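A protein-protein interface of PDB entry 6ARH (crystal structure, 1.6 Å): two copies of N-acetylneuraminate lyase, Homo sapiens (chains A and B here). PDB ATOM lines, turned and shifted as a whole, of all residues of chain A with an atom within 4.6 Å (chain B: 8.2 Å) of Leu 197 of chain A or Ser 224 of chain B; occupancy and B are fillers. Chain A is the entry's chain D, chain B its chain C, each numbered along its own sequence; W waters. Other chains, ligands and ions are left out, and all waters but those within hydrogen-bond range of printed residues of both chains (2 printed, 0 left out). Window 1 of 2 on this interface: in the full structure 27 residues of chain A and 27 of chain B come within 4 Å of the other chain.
OG1 of Thr 195 of chain B is in hydrogen-bond range of OG1 of Thr 195 of chain A, at 2.8 Å. N of Leu 197 of chain B is in hydrogen-bond range of OE1 of Gln 221 of chain A (3.0 Å). OE1 of Gln 221 of chain B sits at hydrogen-bond distance from N of Leu 197 of chain A, at 3.0 Å. NE2 of Gln 268 of chain B lies within hydrogen-bond range of O of Leu 197 of chain A (3.2 Å). The side-chain amide oxygen of Gln 221 of chain B sits close to the backbone carbonyl oxygen of Thr 195 of chain A (3.5 Å).
CD1 of Leu 197 of chain A touches CB of Ser 224 of chain B, at 3.4 Å. CG of Glu 220 of chain B touches CB of Leu 198 of chain A, at 3.97 Å. Gly 201 of chain A touches Gln 268 of chain B (C to OE1, 3.6 Å). O of Thr 195 of chain B touches OE1 of Gln 221 of chain A, at 3.5 Å. CB of Ser 224 of chain A touches CD1 of Leu 197 of chain B, 3.5 Å away. Ser 224 of chain A touches Val 227 of chain B (CA to CG1, 3.9 Å). Leu 223 of chain B touches Val 227 of chain A. Val 227 of chain A touches Ser 224 of chain B (CG1 to CA, 3.9 Å). Met 228 of chain A touches Phe 265 of chain B (O to CZ, 3.7 Å). Gln 268 of chain B touches Met 228 of chain A.
Asp 196 of chain A touches none of the printed residues of chain B. Leu 197 of chain A touches three residues of chain B. Of the printed residues of chain A, Thr 195 of chain B touches Thr 195 (2.8 Å) and Gln 221 (3.5 Å). Of chain A, only Leu 197 (3.4 Å), Ser 224 (3.6 Å) and Val 227 (3.9 Å) come within 4 Å of Ser 224 of chain B. Printed residues of chain A within 4 Å of Phe 265 of chain B: Gly 201 and Met 228. The nearest residue of chain A that does not touch Ser 224 of chain B is Met 228 of chain A (4.1 Å).
The side-chain carboxylate (OD1) of Asp 196 of chain A lies within hydrogen-bond range of the backbone NH (N) of Leu 198 of chain A (3.0 Å). The backbone carbonyl oxygen (O) of Gln 221 of chain B is in hydrogen-bond range of the side-chain hydroxyl (OG) of Ser 224 of chain B. The side-chain amide nitrogen (NE2) of Gln 268 of chain B lies within hydrogen-bond range of the backbone carbonyl oxygen (O) of Glu 220 of chain B (2.8 Å). The side-chain hydroxyl (OG) of Ser 224 of chain A is in hydrogen-bond range of the backbone carbonyl oxygen (O) of Gln 221 of chain A (2.6 Å). The backbone NH (N) of Leu 223 of chain B lies within hydrogen-bond range of the side-chain amide oxygen (OE1) of Gln 264 of chain B (2.8 Å).
Of the 13 printed residues of chain A, 8 touch a printed residue of chain B. Printed residues of chain A that touch a printed residue of chain B: Thr 195, Leu 197, Leu 198, Gly 201, Gln 221, Ser 224, Val 227 and Met 228. Hydrophobic or aromatic side chains of chain A within 4 Å of the printed part of chain B: Leu 197, Leu 198, Val 227 and Met 228.
Thr 195 of chain A touches Gln 221 of chain B, and with the chains exchanged Gln 221 of chain A touches Thr 195 of chain B. Leu 197 of chain A touches Gln 221 of chain B, and with the chains exchanged Gln 221 of chain A touches Leu 197 of chain B. Ser 224 of chain A touches Val 227 of chain B, and with the chains exchanged Val 227 of chain A touches Ser 224 of chain B. Val 227 of chain A touches its own counterpart, Val 227 of chain B. 10 positions are printed for both chains. Of the 21 pairs that touch across the chains among the printed residues, 11 have their exchanged pair printed and touching as well.
Water W1 lies within hydrogen-bond range of O of Thr 195 of chain B (2.5 Å), O of Thr 195 of chain A (2.6 Å), NE2 of Gln 221 of chain A (2.9 Å) and NE2 of Gln 221 of chain B (2.9 Å). Water W2 lies within hydrogen-bond range of the side-chain amide oxygen (OE1) of Gln 221 of chain B (2.7 Å), the side-chain carboxylate (OD1) of Asp 196 of chain A (2.9 Å) and the backbone NH (N) of Leu 198 of chain A (3.5 Å).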
ATOM      1  N   THR A 195     -15.418  38.915 -21.368  1.00  0.00           N
ATOM      2  CA  THR A 195     -15.374  37.445 -21.437  1.00  0.00           C
ATOM      3  C   THR A 195     -15.323  36.764 -20.061  1.00  0.00           C
ATOM      4  O   THR A 195     -15.218  35.534 -19.982  1.00  0.00           O
ATOM      5  CB  THR A 195     -14.196  36.947 -22.304  1.00  0.00           C
ATOM      6  OG1 THR A 195     -12.958  37.324 -21.708  1.00  0.00           O
ATOM      7  CG2 THR A 195     -14.264  37.518 -23.686  1.00  0.00           C
ATOM      8  N   ASP A 196     -15.402  37.536 -18.983  1.00  0.00           N
ATOM      9  CA  ASP A 196     -15.349  36.980 -17.638  1.00  0.00           C
ATOM     10  C   ASP A 196     -16.711  36.401 -17.279  1.00  0.00           C
ATOM     11  O   ASP A 196     -17.604  37.117 -16.837  1.00  0.00           O
ATOM     12  CB  ASP A 196     -14.919  38.040 -16.628  1.00  0.00           C
ATOM     13  CG  ASP A 196     -14.791  37.492 -15.227  1.00  0.00           C
ATOM     14  OD1 ASP A 196     -15.306  36.390 -14.935  1.00  0.00           O
ATOM     15  OD2 ASP A 196     -14.150  38.174 -14.404  1.00  0.00           O
ATOM     16  N   LEU A 197     -16.848  35.085 -17.441  1.00  0.00           N
ATOM     17  CA  LEU A 197     -18.139  34.450 -17.239  1.00  0.00           C
ATOM     18  C   LEU A 197     -18.380  34.025 -15.797  1.00  0.00           C
ATOM     19  O   LEU A 197     -19.467  33.527 -15.488  1.00  0.00           O
ATOM     20  CB  LEU A 197     -18.327  33.304 -18.219  1.00  0.00           C
ATOM     21  CG  LEU A 197     -18.304  33.728 -19.691  1.00  0.00           C
ATOM     22  CD1 LEU A 197     -18.496  32.527 -20.593  1.00  0.00           C
ATOM     23  CD2 LEU A 197     -19.367  34.779 -20.002  1.00  0.00           C
ATOM     24  N   LEU A 198     -17.410  34.225 -14.900  1.00  0.00           N
ATOM     25  CA  LEU A 198     -17.712  34.170 -13.461  1.00  0.00           C
ATOM     26  C   LEU A 198     -18.564  35.378 -13.091  1.00  0.00           C
ATOM     27  O   LEU A 198     -19.615  35.241 -12.425  1.00  0.00           O
ATOM     28  CB  LEU A 198     -16.450  34.116 -12.601  1.00  0.00           C
ATOM     29  CG  LEU A 198     -16.697  34.163 -11.084  1.00  0.00           C
ATOM     30  CD1 LEU A 198     -17.638  33.045 -10.623  1.00  0.00           C
ATOM     31  CD2 LEU A 198     -15.371  34.156 -10.320  1.00  0.00           C
ATOM     32  N   ASP A 199     -18.125  36.555 -13.549  1.00  0.00           N
ATOM     33  CA  ASP A 199     -18.882  37.786 -13.355  1.00  0.00           C
ATOM     34  C   ASP A 199     -20.271  37.655 -14.011  1.00  0.00           C
ATOM     35  O   ASP A 199     -21.287  37.821 -13.347  1.00  0.00           O
ATOM     36  CB  ASP A 199     -18.080  38.986 -13.897  1.00  0.00           C
ATOM     37  CG  ASP A 199     -18.667  40.345 -13.498  1.00  0.00           C
ATOM     38  OD1 ASP A 199     -19.670  40.383 -12.754  1.00  0.00           O
ATOM     39  OD2 ASP A 199     -18.133  41.396 -13.949  1.00  0.00           O
ATOM     40  N   PHE A 200     -20.312  37.280 -15.288  1.00  0.00           N
ATOM     41  CA  PHE A 200     -21.583  37.182 -15.992  1.00  0.00           C
ATOM     42  C   PHE A 200     -22.494  36.128 -15.375  1.00  0.00           C
ATOM     43  O   PHE A 200     -23.673  36.388 -15.141  1.00  0.00           O
ATOM     44  CB  PHE A 200     -21.368  36.875 -17.470  1.00  0.00           C
ATOM     45  CG  PHE A 200     -22.639  36.867 -18.272  1.00  0.00           C
ATOM     46  CD1 PHE A 200     -23.266  38.066 -18.594  1.00  0.00           C
ATOM     47  CD2 PHE A 200     -23.211  35.686 -18.680  1.00  0.00           C
ATOM     48  CE1 PHE A 200     -24.447  38.080 -19.338  1.00  0.00           C
ATOM     49  CE2 PHE A 200     -24.384  35.686 -19.424  1.00  0.00           C
ATOM     50  CZ  PHE A 200     -25.009  36.883 -19.746  1.00  0.00           C
ATOM     51  N   GLY A 201     -21.943  34.949 -15.108  1.00  0.00           N
ATOM     52  CA  GLY A 201     -22.678  33.874 -14.453  1.00  0.00           C
ATOM     53  C   GLY A 201     -23.299  34.304 -13.138  1.00  0.00           C
ATOM     54  O   GLY A 201     -24.445  33.989 -12.879  1.00  0.00           O
ATOM     55  N   PHE A 216     -25.568  39.322 -23.623  1.00  0.00           N
ATOM     56  CA  PHE A 216     -24.141  39.102 -23.751  1.00  0.00           C
ATOM     57  C   PHE A 216     -23.621  39.879 -24.935  1.00  0.00           C
ATOM     58  O   PHE A 216     -24.279  39.928 -25.953  1.00  0.00           O
ATOM     59  CB  PHE A 216     -23.849  37.619 -23.896  1.00  0.00           C
ATOM     60  CG  PHE A 216     -22.394  37.293 -23.790  1.00  0.00           C
ATOM     61  CD1 PHE A 216     -21.711  37.479 -22.603  1.00  0.00           C
ATOM     62  CD2 PHE A 216     -21.713  36.820 -24.889  1.00  0.00           C
ATOM     63  CE1 PHE A 216     -20.365  37.200 -22.509  1.00  0.00           C
ATOM     64  CE2 PHE A 216     -20.369  36.519 -24.805  1.00  0.00           C
ATOM     65  CZ  PHE A 216     -19.695  36.709 -23.614  1.00  0.00           C
ATOM     66  N   GLN A 221     -18.283  34.510 -29.045  1.00  0.00           N
ATOM     67  CA  GLN A 221     -18.447  33.387 -28.126  1.00  0.00           C
ATOM     68  C   GLN A 221     -19.833  33.355 -27.485  1.00  0.00           C
ATOM     69  O   GLN A 221     -19.980  32.935 -26.349  1.00  0.00           O
ATOM     70  CB  GLN A 221     -17.328  33.363 -27.084  1.00  0.00           C
ATOM     71  CG  GLN A 221     -17.255  34.555 -26.149  1.00  0.00           C
ATOM     72  CD  GLN A 221     -16.227  34.353 -25.064  1.00  0.00           C
ATOM     73  OE1 GLN A 221     -15.012  34.533 -25.295  1.00  0.00           O
ATOM     74  NE2 GLN A 221     -16.689  33.964 -23.884  1.00  0.00           N
ATOM     75  N   SER A 224     -21.162  30.232 -25.550  1.00  0.00           N
ATOM     76  CA  SER A 224     -20.586  30.075 -24.213  1.00  0.00           C
ATOM     77  C   SER A 224     -21.354  30.849 -23.145  1.00  0.00           C
ATOM     78  O   SER A 224     -21.375  30.444 -21.985  1.00  0.00           O
ATOM     79  CB  SER A 224     -19.113  30.489 -24.214  1.00  0.00           C
ATOM     80  OG  SER A 224     -18.934  31.902 -24.219  1.00  0.00           O
ATOM     81  N   ALA A 225     -21.932  31.983 -23.521  1.00  0.00           N
ATOM     82  CA  ALA A 225     -22.798  32.743 -22.630  1.00  0.00           C
ATOM     83  C   ALA A 225     -24.219  32.201 -22.553  1.00  0.00           C
ATOM     84  O   ALA A 225     -24.838  32.275 -21.497  1.00  0.00           O
ATOM     85  CB  ALA A 225     -22.827  34.192 -23.051  1.00  0.00           C
ATOM     86  N   VAL A 227     -25.034  29.068 -22.537  1.00  0.00           N
ATOM     87  CA  VAL A 227     -25.003  27.977 -21.562  1.00  0.00           C
ATOM     88  C   VAL A 227     -24.923  28.490 -20.116  1.00  0.00           C
ATOM     89  O   VAL A 227     -25.312  27.783 -19.193  1.00  0.00           O
ATOM     90  CB  VAL A 227     -23.893  26.942 -21.878  1.00  0.00           C
ATOM     91  CG1 VAL A 227     -22.529  27.388 -21.371  1.00  0.00           C
ATOM     92  CG2 VAL A 227     -24.261  25.588 -21.313  1.00  0.00           C
ATOM     93  N   MET A 228     -24.457  29.734 -19.938  1.00  0.00           N
ATOM     94  CA  MET A 228     -24.379  30.379 -18.628  1.00  0.00           C
ATOM     95  C   MET A 228     -25.602  31.210 -18.258  1.00  0.00           C
ATOM     96  O   MET A 228     -25.606  31.873 -17.218  1.00  0.00           O
ATOM     97  CB  MET A 228     -23.131  31.276 -18.570  1.00  0.00           C
ATOM     98  CG  MET A 228     -21.829  30.526 -18.719  1.00  0.00           C
ATOM     99  SD  MET A 228     -21.571  29.243 -17.485  1.00  0.00           S
ATOM    100  CE  MET A 228     -21.655  30.221 -15.984  1.00  0.00           C
ATOM    101  N   ASP B 194      -7.272  30.904 -19.885  1.00  0.00           N
ATOM    102  CA  ASP B 194      -7.589  32.184 -20.508  1.00  0.00           C
ATOM    103  C   ASP B 194      -9.098  32.117 -20.747  1.00  0.00           C
ATOM    104  O   ASP B 194      -9.655  31.021 -20.862  1.00  0.00           O
ATOM    105  CB  ASP B 194      -6.744  32.264 -21.795  1.00  0.00           C
ATOM    106  CG  ASP B 194      -6.965  33.501 -22.646  1.00  0.00           C
ATOM    107  OD1 ASP B 194      -7.816  34.360 -22.401  1.00  0.00           O
ATOM    108  OD2 ASP B 194      -6.200  33.600 -23.633  1.00  0.00           O
ATOM    109  N   THR B 195      -9.761  33.264 -20.788  1.00  0.00           N
ATOM    110  CA  THR B 195     -11.210  33.290 -20.973  1.00  0.00           C
ATOM    111  C   THR B 195     -11.628  33.648 -22.397  1.00  0.00           C
ATOM    112  O   THR B 195     -12.813  33.778 -22.667  1.00  0.00           O
ATOM    113  CB  THR B 195     -11.892  34.245 -19.976  1.00  0.00           C
ATOM    114  OG1 THR B 195     -11.367  35.562 -20.152  1.00  0.00           O
ATOM    115  CG2 THR B 195     -11.650  33.788 -18.551  1.00  0.00           C
ATOM    116  N   LEU B 197     -12.744  32.622 -25.496  1.00  0.00           N
ATOM    117  CA  LEU B 197     -13.289  31.393 -26.071  1.00  0.00           C
ATOM    118  C   LEU B 197     -13.453  31.436 -27.590  1.00  0.00           C
ATOM    119  O   LEU B 197     -13.796  30.416 -28.188  1.00  0.00           O
ATOM    120  CB  LEU B 197     -14.583  30.990 -25.369  1.00  0.00           C
ATOM    121  CG  LEU B 197     -14.438  30.773 -23.873  1.00  0.00           C
ATOM    122  CD1 LEU B 197     -15.758  30.339 -23.237  1.00  0.00           C
ATOM    123  CD2 LEU B 197     -13.339  29.755 -23.583  1.00  0.00           C
ATOM    124  N   PHE B 200     -10.038  29.712 -27.803  1.00  0.00           N
ATOM    125  CA  PHE B 200     -10.200  28.318 -27.406  1.00  0.00           C
ATOM    126  C   PHE B 200     -11.055  27.531 -28.399  1.00  0.00           C
ATOM    127  O   PHE B 200     -10.708  26.419 -28.786  1.00  0.00           O
ATOM    128  CB  PHE B 200     -10.823  28.209 -26.006  1.00  0.00           C
ATOM    129  CG  PHE B 200     -10.913  26.795 -25.506  1.00  0.00           C
ATOM    130  CD1 PHE B 200      -9.784  26.130 -25.075  1.00  0.00           C
ATOM    131  CD2 PHE B 200     -12.131  26.119 -25.492  1.00  0.00           C
ATOM    132  CE1 PHE B 200      -9.844  24.821 -24.623  1.00  0.00           C
ATOM    133  CE2 PHE B 200     -12.204  24.806 -25.024  1.00  0.00           C
ATOM    134  CZ  PHE B 200     -11.062  24.161 -24.580  1.00  0.00           C
ATOM    135  N   GLY B 201     -12.176  28.113 -28.790  1.00  0.00           N
ATOM    136  CA  GLY B 201     -13.070  27.512 -29.752  1.00  0.00           C
ATOM    137  C   GLY B 201     -12.352  27.179 -31.046  1.00  0.00           C
ATOM    138  O   GLY B 201     -12.534  26.092 -31.609  1.00  0.00           O
ATOM    139  N   PHE B 216      -9.430  22.840 -20.516  1.00  0.00           N
ATOM    140  CA  PHE B 216      -9.716  24.179 -20.071  1.00  0.00           C
ATOM    141  C   PHE B 216      -9.195  24.396 -18.657  1.00  0.00           C
ATOM    142  O   PHE B 216      -9.316  23.536 -17.791  1.00  0.00           O
ATOM    143  CB  PHE B 216     -11.206  24.484 -20.161  1.00  0.00           C
ATOM    144  CG  PHE B 216     -11.518  25.936 -20.026  1.00  0.00           C
ATOM    145  CD1 PHE B 216     -11.080  26.850 -20.986  1.00  0.00           C
ATOM    146  CD2 PHE B 216     -12.297  26.393 -18.978  1.00  0.00           C
ATOM    147  CE1 PHE B 216     -11.394  28.193 -20.876  1.00  0.00           C
ATOM    148  CE2 PHE B 216     -12.611  27.727 -18.867  1.00  0.00           C
ATOM    149  CZ  PHE B 216     -12.156  28.627 -19.812  1.00  0.00           C
ATOM    150  N   VAL B 218      -9.773  27.403 -16.592  1.00  0.00           N
ATOM    151  CA  VAL B 218     -10.434  28.407 -15.737  1.00  0.00           C
ATOM    152  C   VAL B 218     -11.651  27.760 -15.087  1.00  0.00           C
ATOM    153  O   VAL B 218     -12.772  27.823 -15.606  1.00  0.00           O
ATOM    154  CB  VAL B 218     -10.797  29.700 -16.509  1.00  0.00           C
ATOM    155  CG1 VAL B 218     -11.268  30.772 -15.546  1.00  0.00           C
ATOM    156  CG2 VAL B 218      -9.600  30.194 -17.314  1.00  0.00           C
ATOM    157  N   ASP B 219     -11.419  27.164 -13.917  1.00  0.00           N
ATOM    158  CA  ASP B 219     -12.404  26.311 -13.248  1.00  0.00           C
ATOM    159  C   ASP B 219     -13.769  26.989 -13.109  1.00  0.00           C
ATOM    160  O   ASP B 219     -14.814  26.372 -13.348  1.00  0.00           O
ATOM    161  CB  ASP B 219     -11.958  25.918 -11.813  1.00  0.00           C
ATOM    162  CG  ASP B 219     -10.544  25.336 -11.734  1.00  0.00           C
ATOM    163  OD1 ASP B 219      -9.637  25.730 -12.517  1.00  0.00           O
ATOM    164  OD2 ASP B 219     -10.330  24.490 -10.844  1.00  0.00           O
ATOM    165  N   GLU B 220     -13.726  28.258 -12.717  1.00  0.00           N
ATOM    166  CA  GLU B 220     -14.933  29.018 -12.378  1.00  0.00           C
ATOM    167  C   GLU B 220     -15.889  29.233 -13.555  1.00  0.00           C
ATOM    168  O   GLU B 220     -17.009  29.672 -13.342  1.00  0.00           O
ATOM    169  CB  GLU B 220     -14.592  30.382 -11.722  1.00  0.00           C
ATOM    170  CG  GLU B 220     -13.644  31.304 -12.492  1.00  0.00           C
ATOM    171  CD  GLU B 220     -12.187  31.157 -12.058  1.00  0.00           C
ATOM    172  OE1 GLU B 220     -11.495  32.197 -12.005  1.00  0.00           O
ATOM    173  OE2 GLU B 220     -11.735  29.998 -11.787  1.00  0.00           O
ATOM    174  N   GLN B 221     -15.459  28.939 -14.781  1.00  0.00           N
ATOM    175  CA  GLN B 221     -16.386  28.972 -15.909  1.00  0.00           C
ATOM    176  C   GLN B 221     -16.197  27.756 -16.822  1.00  0.00           C
ATOM    177  O   GLN B 221     -16.365  27.847 -18.047  1.00  0.00           O
ATOM    178  CB  GLN B 221     -16.266  30.299 -16.667  1.00  0.00           C
ATOM    179  CG  GLN B 221     -14.901  30.542 -17.288  1.00  0.00           C
ATOM    180  CD  GLN B 221     -14.924  31.755 -18.206  1.00  0.00           C
ATOM    181  OE1 GLN B 221     -14.830  32.902 -17.748  1.00  0.00           O
ATOM    182  NE2 GLN B 221     -15.093  31.512 -19.505  1.00  0.00           N
ATOM    183  N   LEU B 222     -15.874  26.605 -16.231  1.00  0.00           N
ATOM    184  CA  LEU B 222     -15.679  25.384 -17.002  1.00  0.00           C
ATOM    185  C   LEU B 222     -16.820  25.053 -17.970  1.00  0.00           C
ATOM    186  O   LEU B 222     -16.568  24.698 -19.124  1.00  0.00           O
ATOM    187  CB  LEU B 222     -15.401  24.187 -16.098  1.00  0.00           C
ATOM    188  CG  LEU B 222     -15.229  22.821 -16.759  1.00  0.00           C
ATOM    189  CD1 LEU B 222     -14.173  22.848 -17.866  1.00  0.00           C
ATOM    190  CD2 LEU B 222     -14.906  21.758 -15.724  1.00  0.00           C
ATOM    191  N   LEU B 223     -18.065  25.182 -17.512  1.00  0.00           N
ATOM    192  CA  LEU B 223     -19.200  24.821 -18.362  1.00  0.00           C
ATOM    193  C   LEU B 223     -19.169  25.579 -19.690  1.00  0.00           C
ATOM    194  O   LEU B 223     -19.493  25.024 -20.757  1.00  0.00           O
ATOM    195  CB  LEU B 223     -20.517  25.085 -17.627  1.00  0.00           C
ATOM    196  CG  LEU B 223     -21.793  24.713 -18.390  1.00  0.00           C
ATOM    197  CD1 LEU B 223     -21.826  23.251 -18.801  1.00  0.00           C
ATOM    198  CD2 LEU B 223     -22.996  25.072 -17.536  1.00  0.00           C
ATOM    199  N   SER B 224     -18.769  26.847 -19.629  1.00  0.00           N
ATOM    200  CA  SER B 224     -18.696  27.671 -20.845  1.00  0.00           C
ATOM    201  C   SER B 224     -17.693  27.139 -21.868  1.00  0.00           C
ATOM    202  O   SER B 224     -17.886  27.343 -23.046  1.00  0.00           O
ATOM    203  CB  SER B 224     -18.377  29.120 -20.483  1.00  0.00           C
ATOM    204  OG  SER B 224     -17.015  29.277 -20.091  1.00  0.00           O
ATOM    205  N   ALA B 225     -16.631  26.474 -21.410  1.00  0.00           N
ATOM    206  CA  ALA B 225     -15.663  25.847 -22.305  1.00  0.00           C
ATOM    207  C   ALA B 225     -16.093  24.455 -22.755  1.00  0.00           C
ATOM    208  O   ALA B 225     -15.800  24.056 -23.870  1.00  0.00           O
ATOM    209  CB  ALA B 225     -14.304  25.776 -21.645  1.00  0.00           C
ATOM    210  N   LEU B 226     -16.774  23.721 -21.879  1.00  0.00           N
ATOM    211  CA  LEU B 226     -17.327  22.418 -22.262  1.00  0.00           C
ATOM    212  C   LEU B 226     -18.221  22.567 -23.487  1.00  0.00           C
ATOM    213  O   LEU B 226     -18.120  21.779 -24.416  1.00  0.00           O
ATOM    214  CB  LEU B 226     -18.113  21.806 -21.116  1.00  0.00           C
ATOM    215  CG  LEU B 226     -17.296  21.374 -19.880  1.00  0.00           C
ATOM    216  CD1 LEU B 226     -18.252  20.871 -18.813  1.00  0.00           C
ATOM    217  CD2 LEU B 226     -16.252  20.326 -20.237  1.00  0.00           C
ATOM    218  N   VAL B 227     -19.078  23.589 -23.504  1.00  0.00           N
ATOM    219  CA  VAL B 227     -20.015  23.726 -24.632  1.00  0.00           C
ATOM    220  C   VAL B 227     -19.287  24.071 -25.932  1.00  0.00           C
ATOM    221  O   VAL B 227     -19.794  23.798 -27.020  1.00  0.00           O
ATOM    222  CB  VAL B 227     -21.144  24.745 -24.346  1.00  0.00           C
ATOM    223  CG1 VAL B 227     -20.661  26.191 -24.456  1.00  0.00           C
ATOM    224  CG2 VAL B 227     -22.314  24.517 -25.276  1.00  0.00           C
ATOM    225  N   MET B 228     -18.101  24.652 -25.795  1.00  0.00           N
ATOM    226  CA  MET B 228     -17.230  24.985 -26.916  1.00  0.00           C
ATOM    227  C   MET B 228     -16.268  23.869 -27.328  1.00  0.00           C
ATOM    228  O   MET B 228     -15.433  24.087 -28.211  1.00  0.00           O
ATOM    229  CB  MET B 228     -16.449  26.271 -26.581  1.00  0.00           C
ATOM    230  CG  MET B 228     -17.305  27.504 -26.382  1.00  0.00           C
ATOM    231  SD  MET B 228     -18.390  27.900 -27.771  1.00  0.00           S
ATOM    232  CE  MET B 228     -17.185  28.040 -29.086  1.00  0.00           C
ATOM    233  N   GLY B 229     -16.368  22.681 -26.718  1.00  0.00           N
ATOM    234  CA  GLY B 229     -15.602  21.518 -27.150  1.00  0.00           C
ATOM    235  C   GLY B 229     -14.427  21.105 -26.279  1.00  0.00           C
ATOM    236  O   GLY B 229     -13.622  20.252 -26.683  1.00  0.00           O
ATOM    237  N   ALA B 230     -14.311  21.665 -25.076  1.00  0.00           N
ATOM    238  CA  ALA B 230     -13.259  21.219 -24.159  1.00  0.00           C
ATOM    239  C   ALA B 230     -13.372  19.710 -23.923  1.00  0.00           C
ATOM    240  O   ALA B 230     -14.472  19.197 -23.749  1.00  0.00           O
ATOM    241  CB  ALA B 230     -13.333  21.951 -22.831  1.00  0.00           C
ATOM    242  N   MET B 248     -21.456  18.114 -12.589  1.00  0.00           N
ATOM    243  CA  MET B 248     -21.635  19.078 -13.674  1.00  0.00           C
ATOM    244  C   MET B 248     -21.198  18.498 -15.015  1.00  0.00           C
ATOM    245  O   MET B 248     -21.910  18.599 -16.018  1.00  0.00           O
ATOM    246  CB  MET B 248     -20.912  20.400 -13.382  1.00  0.00           C
ATOM    247  CG  MET B 248     -20.969  21.404 -14.537  1.00  0.00           C
ATOM    248  SD  MET B 248     -20.047  22.866 -14.106  1.00  0.00           S
ATOM    249  CE  MET B 248     -18.381  22.301 -14.469  1.00  0.00           C
ATOM    250  N   PHE B 252     -23.547  17.779 -18.223  1.00  0.00           N
ATOM    251  CA  PHE B 252     -23.197  18.274 -19.547  1.00  0.00           C
ATOM    252  C   PHE B 252     -23.145  17.170 -20.608  1.00  0.00           C
ATOM    253  O   PHE B 252     -23.692  17.322 -21.716  1.00  0.00           O
ATOM    254  CB  PHE B 252     -21.859  19.023 -19.514  1.00  0.00           C
ATOM    255  CG  PHE B 252     -21.352  19.356 -20.866  1.00  0.00           C
ATOM    256  CD1 PHE B 252     -21.864  20.448 -21.548  1.00  0.00           C
ATOM    257  CD2 PHE B 252     -20.394  18.550 -21.488  1.00  0.00           C
ATOM    258  CE1 PHE B 252     -21.445  20.731 -22.842  1.00  0.00           C
ATOM    259  CE2 PHE B 252     -19.963  18.844 -22.765  1.00  0.00           C
ATOM    260  CZ  PHE B 252     -20.490  19.935 -23.434  1.00  0.00           C
ATOM    261  N   LEU B 261     -25.752  23.890 -15.443  1.00  0.00           N
ATOM    262  CA  LEU B 261     -25.577  25.294 -15.085  1.00  0.00           C
ATOM    263  C   LEU B 261     -25.804  25.481 -13.592  1.00  0.00           C
ATOM    264  O   LEU B 261     -25.048  26.188 -12.935  1.00  0.00           O
ATOM    265  CB  LEU B 261     -26.498  26.191 -15.910  1.00  0.00           C
ATOM    266  CG  LEU B 261     -26.461  27.677 -15.547  1.00  0.00           C
ATOM    267  CD1 LEU B 261     -25.041  28.216 -15.697  1.00  0.00           C
ATOM    268  CD2 LEU B 261     -27.452  28.447 -16.390  1.00  0.00           C
ATOM    269  N   GLN B 264     -22.711  24.342 -11.936  1.00  0.00           N
ATOM    270  CA  GLN B 264     -21.683  25.364 -12.158  1.00  0.00           C
ATOM    271  C   GLN B 264     -21.862  26.542 -11.223  1.00  0.00           C
ATOM    272  O   GLN B 264     -20.885  27.042 -10.663  1.00  0.00           O
ATOM    273  CB  GLN B 264     -21.688  25.883 -13.592  1.00  0.00           C
ATOM    274  CG  GLN B 264     -20.579  26.891 -13.905  1.00  0.00           C
ATOM    275  CD  GLN B 264     -19.206  26.303 -13.808  1.00  0.00           C
ATOM    276  OE1 GLN B 264     -18.635  25.892 -14.812  1.00  0.00           O
ATOM    277  NE2 GLN B 264     -18.653  26.253 -12.595  1.00  0.00           N
ATOM    278  N   PHE B 265     -23.101  26.985 -11.051  1.00  0.00           N
ATOM    279  CA  PHE B 265     -23.389  28.082 -10.131  1.00  0.00           C
ATOM    280  C   PHE B 265     -23.048  27.766  -8.675  1.00  0.00           C
ATOM    281  O   PHE B 265     -22.585  28.663  -7.970  1.00  0.00           O
ATOM    282  CB  PHE B 265     -24.849  28.539 -10.232  1.00  0.00           C
ATOM    283  CG  PHE B 265     -25.195  29.333 -11.468  1.00  0.00           C
ATOM    284  CD1 PHE B 265     -24.268  30.120 -12.170  1.00  0.00           C
ATOM    285  CD2 PHE B 265     -26.515  29.338 -11.910  1.00  0.00           C
ATOM    286  CE1 PHE B 265     -24.667  30.851 -13.275  1.00  0.00           C
ATOM    287  CE2 PHE B 265     -26.913  30.098 -12.999  1.00  0.00           C
ATOM    288  CZ  PHE B 265     -25.986  30.841 -13.686  1.00  0.00           C
ATOM    289  N   GLN B 268     -19.431  28.359  -8.591  1.00  0.00           N
ATOM    290  CA  GLN B 268     -19.182  29.799  -8.709  1.00  0.00           C
ATOM    291  C   GLN B 268     -19.472  30.565  -7.429  1.00  0.00           C
ATOM    292  O   GLN B 268     -18.773  31.528  -7.105  1.00  0.00           O
ATOM    293  CB  GLN B 268     -19.998  30.409  -9.848  1.00  0.00           C
ATOM    294  CG  GLN B 268     -19.520  30.074 -11.240  1.00  0.00           C
ATOM    295  CD  GLN B 268     -20.127  30.991 -12.292  1.00  0.00           C
ATOM    296  OE1 GLN B 268     -21.153  31.648 -12.059  1.00  0.00           O
ATOM    297  NE2 GLN B 268     -19.479  31.060 -13.457  1.00  0.00           N
HETATM  298  O   HOH W   1     -15.086  33.502 -21.572  1.00  0.00           O
HETATM  299  O   HOH W   2     -13.980  33.875 -15.358  1.00  0.00           O
